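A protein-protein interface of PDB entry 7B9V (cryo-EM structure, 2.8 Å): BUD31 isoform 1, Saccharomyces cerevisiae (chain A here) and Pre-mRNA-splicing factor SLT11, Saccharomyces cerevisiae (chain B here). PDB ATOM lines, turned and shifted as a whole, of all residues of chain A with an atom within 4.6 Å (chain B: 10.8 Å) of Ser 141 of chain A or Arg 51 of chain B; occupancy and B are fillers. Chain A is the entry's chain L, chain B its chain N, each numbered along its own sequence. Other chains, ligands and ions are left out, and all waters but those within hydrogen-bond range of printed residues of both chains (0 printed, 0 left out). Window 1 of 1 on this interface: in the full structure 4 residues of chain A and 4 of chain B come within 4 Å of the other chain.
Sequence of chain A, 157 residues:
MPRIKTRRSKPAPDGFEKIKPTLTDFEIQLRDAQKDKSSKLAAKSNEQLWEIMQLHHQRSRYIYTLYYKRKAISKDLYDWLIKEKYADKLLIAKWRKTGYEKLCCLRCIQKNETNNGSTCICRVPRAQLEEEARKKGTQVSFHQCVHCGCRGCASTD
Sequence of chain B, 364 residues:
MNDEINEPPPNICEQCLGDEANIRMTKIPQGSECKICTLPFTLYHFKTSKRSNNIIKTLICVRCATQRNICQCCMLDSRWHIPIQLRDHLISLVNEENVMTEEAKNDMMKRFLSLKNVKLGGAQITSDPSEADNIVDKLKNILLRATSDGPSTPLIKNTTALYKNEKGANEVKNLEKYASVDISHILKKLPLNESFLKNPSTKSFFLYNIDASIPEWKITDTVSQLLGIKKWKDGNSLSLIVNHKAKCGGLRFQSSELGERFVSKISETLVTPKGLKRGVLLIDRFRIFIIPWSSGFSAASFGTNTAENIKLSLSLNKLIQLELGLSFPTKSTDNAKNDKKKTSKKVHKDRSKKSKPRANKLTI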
ATOM      1  N   ILE A 121     -12.988 -31.144 -28.666  1.00  0.00           N
ATOM      2  CA  ILE A 121     -14.020 -32.181 -28.712  1.00  0.00           C
ATOM      3  C   ILE A 121     -13.978 -32.966 -30.032  1.00  0.00           C
ATOM      4  O   ILE A 121     -14.382 -34.136 -30.064  1.00  0.00           O
ATOM      5  CB  ILE A 121     -15.411 -31.542 -28.444  1.00  0.00           C
ATOM      6  CG1 ILE A 121     -16.548 -32.575 -28.364  1.00  0.00           C
ATOM      7  CG2 ILE A 121     -15.746 -30.603 -29.531  1.00  0.00           C
ATOM      8  CD1 ILE A 121     -17.806 -32.094 -27.663  1.00  0.00           C
ATOM      9  N   LYS A 136     -27.907 -39.817 -22.447  1.00  0.00           N
ATOM     10  CA  LYS A 136     -28.652 -38.639 -22.020  1.00  0.00           C
ATOM     11  C   LYS A 136     -30.029 -38.572 -22.671  1.00  0.00           C
ATOM     12  O   LYS A 136     -30.947 -37.961 -22.115  1.00  0.00           O
ATOM     13  CB  LYS A 136     -27.850 -37.374 -22.327  1.00  0.00           C
ATOM     14  CG  LYS A 136     -26.685 -37.121 -21.369  1.00  0.00           C
ATOM     15  CD  LYS A 136     -26.012 -35.777 -21.635  1.00  0.00           C
ATOM     16  CE  LYS A 136     -26.867 -34.611 -21.166  1.00  0.00           C
ATOM     17  NZ  LYS A 136     -26.156 -33.310 -21.315  1.00  0.00           N
ATOM     18  N   GLN A 139     -29.942 -36.084 -29.436  1.00  0.00           N
ATOM     19  CA  GLN A 139     -28.989 -36.067 -30.539  1.00  0.00           C
ATOM     20  C   GLN A 139     -27.671 -35.428 -30.097  1.00  0.00           C
ATOM     21  O   GLN A 139     -27.570 -34.812 -29.033  1.00  0.00           O
ATOM     22  CB  GLN A 139     -29.562 -35.319 -31.749  1.00  0.00           C
ATOM     23  CG  GLN A 139     -30.729 -36.015 -32.464  1.00  0.00           C
ATOM     24  CD  GLN A 139     -32.073 -35.814 -31.776  1.00  0.00           C
ATOM     25  OE1 GLN A 139     -32.169 -35.134 -30.754  1.00  0.00           O
ATOM     26  NE2 GLN A 139     -33.113 -36.439 -32.318  1.00  0.00           N
ATOM     27  N   VAL A 140     -26.655 -35.567 -30.943  1.00  0.00           N
ATOM     28  CA  VAL A 140     -25.334 -35.014 -30.655  1.00  0.00           C
ATOM     29  C   VAL A 140     -25.338 -33.532 -31.005  1.00  0.00           C
ATOM     30  O   VAL A 140     -25.688 -33.148 -32.126  1.00  0.00           O
ATOM     31  CB  VAL A 140     -24.244 -35.772 -31.426  1.00  0.00           C
ATOM     32  CG1 VAL A 140     -22.872 -35.172 -31.153  1.00  0.00           C
ATOM     33  CG2 VAL A 140     -24.271 -37.231 -31.044  1.00  0.00           C
ATOM     34  N   SER A 141     -24.939 -32.694 -30.046  1.00  0.00           N
ATOM     35  CA  SER A 141     -24.952 -31.249 -30.239  1.00  0.00           C
ATOM     36  C   SER A 141     -23.715 -30.728 -30.961  1.00  0.00           C
ATOM     37  O   SER A 141     -23.741 -29.597 -31.460  1.00  0.00           O
ATOM     38  CB  SER A 141     -25.093 -30.545 -28.888  1.00  0.00           C
ATOM     39  OG  SER A 141     -24.084 -30.973 -27.988  1.00  0.00           O
ATOM     40  N   PHE A 142     -22.637 -31.505 -31.021  1.00  0.00           N
ATOM     41  CA  PHE A 142     -21.401 -31.040 -31.640  1.00  0.00           C
ATOM     42  C   PHE A 142     -21.466 -31.202 -33.155  1.00  0.00           C
ATOM     43  O   PHE A 142     -21.593 -32.321 -33.664  1.00  0.00           O
ATOM     44  CB  PHE A 142     -20.194 -31.790 -31.086  1.00  0.00           C
ATOM     45  CG  PHE A 142     -18.942 -31.564 -31.880  1.00  0.00           C
ATOM     46  CD1 PHE A 142     -18.393 -30.294 -31.977  1.00  0.00           C
ATOM     47  CD2 PHE A 142     -18.324 -32.613 -32.546  1.00  0.00           C
ATOM     48  CE1 PHE A 142     -17.254 -30.079 -32.718  1.00  0.00           C
ATOM     49  CE2 PHE A 142     -17.175 -32.400 -33.292  1.00  0.00           C
ATOM     50  CZ  PHE A 142     -16.643 -31.128 -33.378  1.00  0.00           C
ATOM     51  N   HIS A 143     -21.379 -30.079 -33.871  1.00  0.00           N
ATOM     52  CA  HIS A 143     -21.281 -30.071 -35.328  1.00  0.00           C
ATOM     53  C   HIS A 143     -19.867 -29.757 -35.816  1.00  0.00           C
ATOM     54  O   HIS A 143     -19.250 -30.577 -36.501  1.00  0.00           O
ATOM     55  CB  HIS A 143     -22.292 -29.074 -35.900  1.00  0.00           C
ATOM     56  CG  HIS A 143     -23.675 -29.259 -35.360  1.00  0.00           C
ATOM     57  ND1 HIS A 143     -24.524 -30.250 -35.802  1.00  0.00           N
ATOM     58  CD2 HIS A 143     -24.352 -28.579 -34.406  1.00  0.00           C
ATOM     59  CE1 HIS A 143     -25.666 -30.172 -35.141  1.00  0.00           C
ATOM     60  NE2 HIS A 143     -25.588 -29.167 -34.289  1.00  0.00           N
ATOM     61  N   GLU B  20     -27.073 -32.793 -11.866  1.00  0.00           N
ATOM     62  CA  GLU B  20     -25.776 -33.438 -12.013  1.00  0.00           C
ATOM     63  C   GLU B  20     -25.010 -33.371 -10.701  1.00  0.00           C
ATOM     64  O   GLU B  20     -25.192 -32.441  -9.909  1.00  0.00           O
ATOM     65  CB  GLU B  20     -24.968 -32.782 -13.139  1.00  0.00           C
ATOM     66  CG  GLU B  20     -25.601 -32.861 -14.535  1.00  0.00           C
ATOM     67  CD  GLU B  20     -25.754 -34.281 -15.104  1.00  0.00           C
ATOM     68  OE1 GLU B  20     -25.096 -35.239 -14.637  1.00  0.00           O
ATOM     69  OE2 GLU B  20     -26.580 -34.447 -16.026  1.00  0.00           O
ATOM     70  N   ASN B  22     -21.849 -32.973 -10.110  1.00  0.00           N
ATOM     71  CA  ASN B  22     -20.808 -31.960 -10.074  1.00  0.00           C
ATOM     72  C   ASN B  22     -21.078 -30.880 -11.108  1.00  0.00           C
ATOM     73  O   ASN B  22     -21.474 -31.174 -12.241  1.00  0.00           O
ATOM     74  CB  ASN B  22     -19.425 -32.570 -10.303  1.00  0.00           C
ATOM     75  CG  ASN B  22     -19.042 -33.547  -9.216  1.00  0.00           C
ATOM     76  OD1 ASN B  22     -18.872 -33.166  -8.058  1.00  0.00           O
ATOM     77  ND2 ASN B  22     -18.906 -34.815  -9.580  1.00  0.00           N
ATOM     78  N   ILE B  23     -20.865 -29.631 -10.707  1.00  0.00           N
ATOM     79  CA  ILE B  23     -20.991 -28.469 -11.579  1.00  0.00           C
ATOM     80  C   ILE B  23     -19.686 -27.693 -11.518  1.00  0.00           C
ATOM     81  O   ILE B  23     -19.239 -27.310 -10.430  1.00  0.00           O
ATOM     82  CB  ILE B  23     -22.200 -27.576 -11.229  1.00  0.00           C
ATOM     83  CG1 ILE B  23     -23.523 -28.275 -11.561  1.00  0.00           C
ATOM     84  CG2 ILE B  23     -22.124 -26.219 -11.899  1.00  0.00           C
ATOM     85  CD1 ILE B  23     -24.154 -29.013 -10.467  1.00  0.00           C
ATOM     86  N   ARG B  24     -19.073 -27.473 -12.677  1.00  0.00           N
ATOM     87  CA  ARG B  24     -17.969 -26.533 -12.780  1.00  0.00           C
ATOM     88  C   ARG B  24     -18.525 -25.117 -12.897  1.00  0.00           C
ATOM     89  O   ARG B  24     -19.492 -24.872 -13.624  1.00  0.00           O
ATOM     90  CB  ARG B  24     -17.076 -26.885 -13.970  1.00  0.00           C
ATOM     91  CG  ARG B  24     -15.800 -26.064 -14.058  1.00  0.00           C
ATOM     92  CD  ARG B  24     -15.017 -26.394 -15.323  1.00  0.00           C
ATOM     93  NE  ARG B  24     -14.653 -27.807 -15.418  1.00  0.00           N
ATOM     94  CZ  ARG B  24     -13.674 -28.405 -14.747  1.00  0.00           C
ATOM     95  NH1 ARG B  24     -12.913 -27.747 -13.888  1.00  0.00           N
ATOM     96  NH2 ARG B  24     -13.456 -29.701 -14.945  1.00  0.00           N
ATOM     97  N   PHE B  46     -22.002 -20.719 -14.993  1.00  0.00           N
ATOM     98  CA  PHE B  46     -21.915 -22.165 -15.080  1.00  0.00           C
ATOM     99  C   PHE B  46     -22.896 -22.671 -16.127  1.00  0.00           C
ATOM    100  O   PHE B  46     -23.798 -21.956 -16.567  1.00  0.00           O
ATOM    101  CB  PHE B  46     -22.220 -22.802 -13.708  1.00  0.00           C
ATOM    102  CG  PHE B  46     -23.650 -22.560 -13.211  1.00  0.00           C
ATOM    103  CD1 PHE B  46     -23.976 -21.373 -12.554  1.00  0.00           C
ATOM    104  CD2 PHE B  46     -24.650 -23.513 -13.391  1.00  0.00           C
ATOM    105  CE1 PHE B  46     -25.256 -21.138 -12.104  1.00  0.00           C
ATOM    106  CE2 PHE B  46     -25.939 -23.276 -12.946  1.00  0.00           C
ATOM    107  CZ  PHE B  46     -26.238 -22.087 -12.302  1.00  0.00           C
ATOM    108  N   LYS B  47     -22.715 -23.933 -16.516  1.00  0.00           N
ATOM    109  CA  LYS B  47     -23.689 -24.678 -17.300  1.00  0.00           C
ATOM    110  C   LYS B  47     -24.137 -25.896 -16.506  1.00  0.00           C
ATOM    111  O   LYS B  47     -23.375 -26.423 -15.691  1.00  0.00           O
ATOM    112  CB  LYS B  47     -23.106 -25.112 -18.652  1.00  0.00           C
ATOM    113  CG  LYS B  47     -22.490 -23.985 -19.459  1.00  0.00           C
ATOM    114  CD  LYS B  47     -22.443 -24.316 -20.939  1.00  0.00           C
ATOM    115  CE  LYS B  47     -21.474 -25.443 -21.242  1.00  0.00           C
ATOM    116  NZ  LYS B  47     -21.477 -25.792 -22.690  1.00  0.00           N
ATOM    117  N   THR B  48     -25.402 -26.302 -16.703  1.00  0.00           N
ATOM    118  CA  THR B  48     -25.954 -27.443 -15.967  1.00  0.00           C
ATOM    119  C   THR B  48     -25.243 -28.748 -16.316  1.00  0.00           C
ATOM    120  O   THR B  48     -25.122 -29.638 -15.468  1.00  0.00           O
ATOM    121  CB  THR B  48     -27.455 -27.573 -16.237  1.00  0.00           C
ATOM    122  OG1 THR B  48     -27.696 -27.574 -17.649  1.00  0.00           O
ATOM    123  CG2 THR B  48     -28.215 -26.415 -15.601  1.00  0.00           C
ATOM    124  N   SER B  49     -24.769 -28.874 -17.551  1.00  0.00           N
ATOM    125  CA  SER B  49     -23.914 -29.976 -17.959  1.00  0.00           C
ATOM    126  C   SER B  49     -22.975 -29.427 -19.020  1.00  0.00           C
ATOM    127  O   SER B  49     -23.162 -28.306 -19.499  1.00  0.00           O
ATOM    128  CB  SER B  49     -24.728 -31.160 -18.490  1.00  0.00           C
ATOM    129  OG  SER B  49     -25.392 -30.819 -19.697  1.00  0.00           O
ATOM    130  N   LYS B  50     -21.919 -30.202 -19.319  1.00  0.00           N
ATOM    131  CA  LYS B  50     -20.856 -29.753 -20.224  1.00  0.00           C
ATOM    132  C   LYS B  50     -21.395 -29.482 -21.628  1.00  0.00           C
ATOM    133  O   LYS B  50     -20.947 -28.555 -22.313  1.00  0.00           O
ATOM    134  CB  LYS B  50     -19.726 -30.785 -20.267  1.00  0.00           C
ATOM    135  CG  LYS B  50     -18.806 -30.798 -19.032  1.00  0.00           C
ATOM    136  CD  LYS B  50     -18.041 -29.493 -18.811  1.00  0.00           C
ATOM    137  CE  LYS B  50     -17.054 -29.183 -19.931  1.00  0.00           C
ATOM    138  NZ  LYS B  50     -15.938 -30.175 -20.003  1.00  0.00           N
ATOM    139  N   ARG B  51     -22.353 -30.297 -22.072  1.00  0.00           N
ATOM    140  CA  ARG B  51     -22.878 -30.228 -23.427  1.00  0.00           C
ATOM    141  C   ARG B  51     -24.219 -29.514 -23.536  1.00  0.00           C
ATOM    142  O   ARG B  51     -24.792 -29.480 -24.629  1.00  0.00           O
ATOM    143  CB  ARG B  51     -22.973 -31.636 -24.024  1.00  0.00           C
ATOM    144  CG  ARG B  51     -21.612 -32.340 -24.180  1.00  0.00           C
ATOM    145  CD  ARG B  51     -20.769 -31.881 -25.399  1.00  0.00           C
ATOM    146  NE  ARG B  51     -20.124 -30.578 -25.239  1.00  0.00           N
ATOM    147  CZ  ARG B  51     -18.990 -30.365 -24.583  1.00  0.00           C
ATOM    148  NH1 ARG B  51     -18.332 -31.353 -24.003  1.00  0.00           N
ATOM    149  NH2 ARG B  51     -18.524 -29.123 -24.477  1.00  0.00           N
ATOM    150  N   SER B  52     -24.736 -28.946 -22.450  1.00  0.00           N
ATOM    151  CA  SER B  52     -25.829 -27.990 -22.573  1.00  0.00           C
ATOM    152  C   SER B  52     -25.326 -26.698 -23.207  1.00  0.00           C
ATOM    153  O   SER B  52     -24.194 -26.275 -22.975  1.00  0.00           O
ATOM    154  CB  SER B  52     -26.448 -27.714 -21.202  1.00  0.00           C
ATOM    155  OG  SER B  52     -26.928 -28.912 -20.613  1.00  0.00           O
ATOM    156  N   ASN B  53     -26.168 -26.082 -24.035  1.00  0.00           N
ATOM    157  CA  ASN B  53     -25.722 -24.998 -24.898  1.00  0.00           C
ATOM    158  C   ASN B  53     -26.080 -23.617 -24.354  1.00  0.00           C
ATOM    159  O   ASN B  53     -25.649 -22.610 -24.924  1.00  0.00           O
ATOM    160  CB  ASN B  53     -26.323 -25.181 -26.301  1.00  0.00           C
ATOM    161  CG  ASN B  53     -25.506 -24.510 -27.386  1.00  0.00           C
ATOM    162  OD1 ASN B  53     -24.277 -24.578 -27.389  1.00  0.00           O
ATOM    163  ND2 ASN B  53     -26.189 -23.859 -28.319  1.00  0.00           N
ATOM    164  N   ASN B  54     -26.833 -23.543 -23.263  1.00  0.00           N
ATOM    165  CA  ASN B  54     -27.153 -22.282 -22.609  1.00  0.00           C
ATOM    166  C   ASN B  54     -26.301 -22.088 -21.358  1.00  0.00           C
ATOM    167  O   ASN B  54     -26.099 -23.015 -20.569  1.00  0.00           O
ATOM    168  CB  ASN B  54     -28.651 -22.211 -22.302  1.00  0.00           C
ATOM    169  CG  ASN B  54     -29.118 -23.321 -21.382  1.00  0.00           C
ATOM    170  OD1 ASN B  54     -28.972 -24.499 -21.701  1.00  0.00           O
ATOM    171  ND2 ASN B  54     -29.726 -22.947 -20.272  1.00  0.00           N
ATOM    172  N   ILE B  55     -25.768 -20.878 -21.209  1.00  0.00           N
ATOM    173  CA  ILE B  55     -24.829 -20.529 -20.148  1.00  0.00           C
ATOM    174  C   ILE B  55     -25.514 -19.601 -19.140  1.00  0.00           C
ATOM    175  O   ILE B  55     -26.015 -18.528 -19.503  1.00  0.00           O
ATOM    176  CB  ILE B  55     -23.533 -19.949 -20.743  1.00  0.00           C
ATOM    177  CG1 ILE B  55     -22.623 -19.380 -19.671  1.00  0.00           C
ATOM    178  CG2 ILE B  55     -23.819 -18.954 -21.878  1.00  0.00           C
ATOM    179  CD1 ILE B  55     -21.293 -19.046 -20.251  1.00  0.00           C
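A ring nitrogen (NE2) of His 143 of chain A lies close to the backbone carbonyl oxygen (O) of Ser 141 of chain A, 3.4 Å away.
The side-chain hydroxyl (OG) of Ser 49 of chain B is in hydrogen-bond range of the side-chain hydroxyl (OG) of Ser 52 of chain B, at 2.6 Å.
Of the 7 printed residues of chain A, 3 touch a printed residue of chain B.
Printed residues of chain A that touch a printed residue of chain B: Ile 121, Lys 136 and Ser 141.
Hydrophobic or aromatic side chains of chain A within 4 Å of the printed part of chain B: Ile 121.
Of the 14 printed residues of chain B, 2 touch a printed residue of chain A.
NZ of Lys 136 of chain A sits at hydrogen-bond distance from OG of Ser 49 of chain B, at 3.1 Å.
Of the printed residues of chain A, Arg 51 of chain B touches Ile 121 and Ser 141.
Of the printed residues of chain A, Ser 49 of chain B touches Lys 136 (3.1 Å).
Of the printed residues of chain B, Lys 136 of chain A touches Ser 49.
Printed residues of chain B within 4 Å of Ile 121 of chain A: Arg 51 (3.7 Å).
Asn 53 of chain B touches none of the printed residues of chain A.
The nearest residue of chain B that does not touch Ser 141 of chain A is Ser 52 of chain B (5.9 Å).
The nearest residue of chain A that does not touch Arg 51 of chain B is Lys 136 of chain A (4.5 Å).
The nearest printed residue of chain B that does not touch Lys 136 of chain A is Arg 51 of chain B (4.5 Å).
Among the printed residues, merely in contact across the chains: Ile 121 of chain A with Arg 51 of chain B (3.7 Å) and Ser 141 of chain A with Arg 51 of chain B (3.7 Å).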
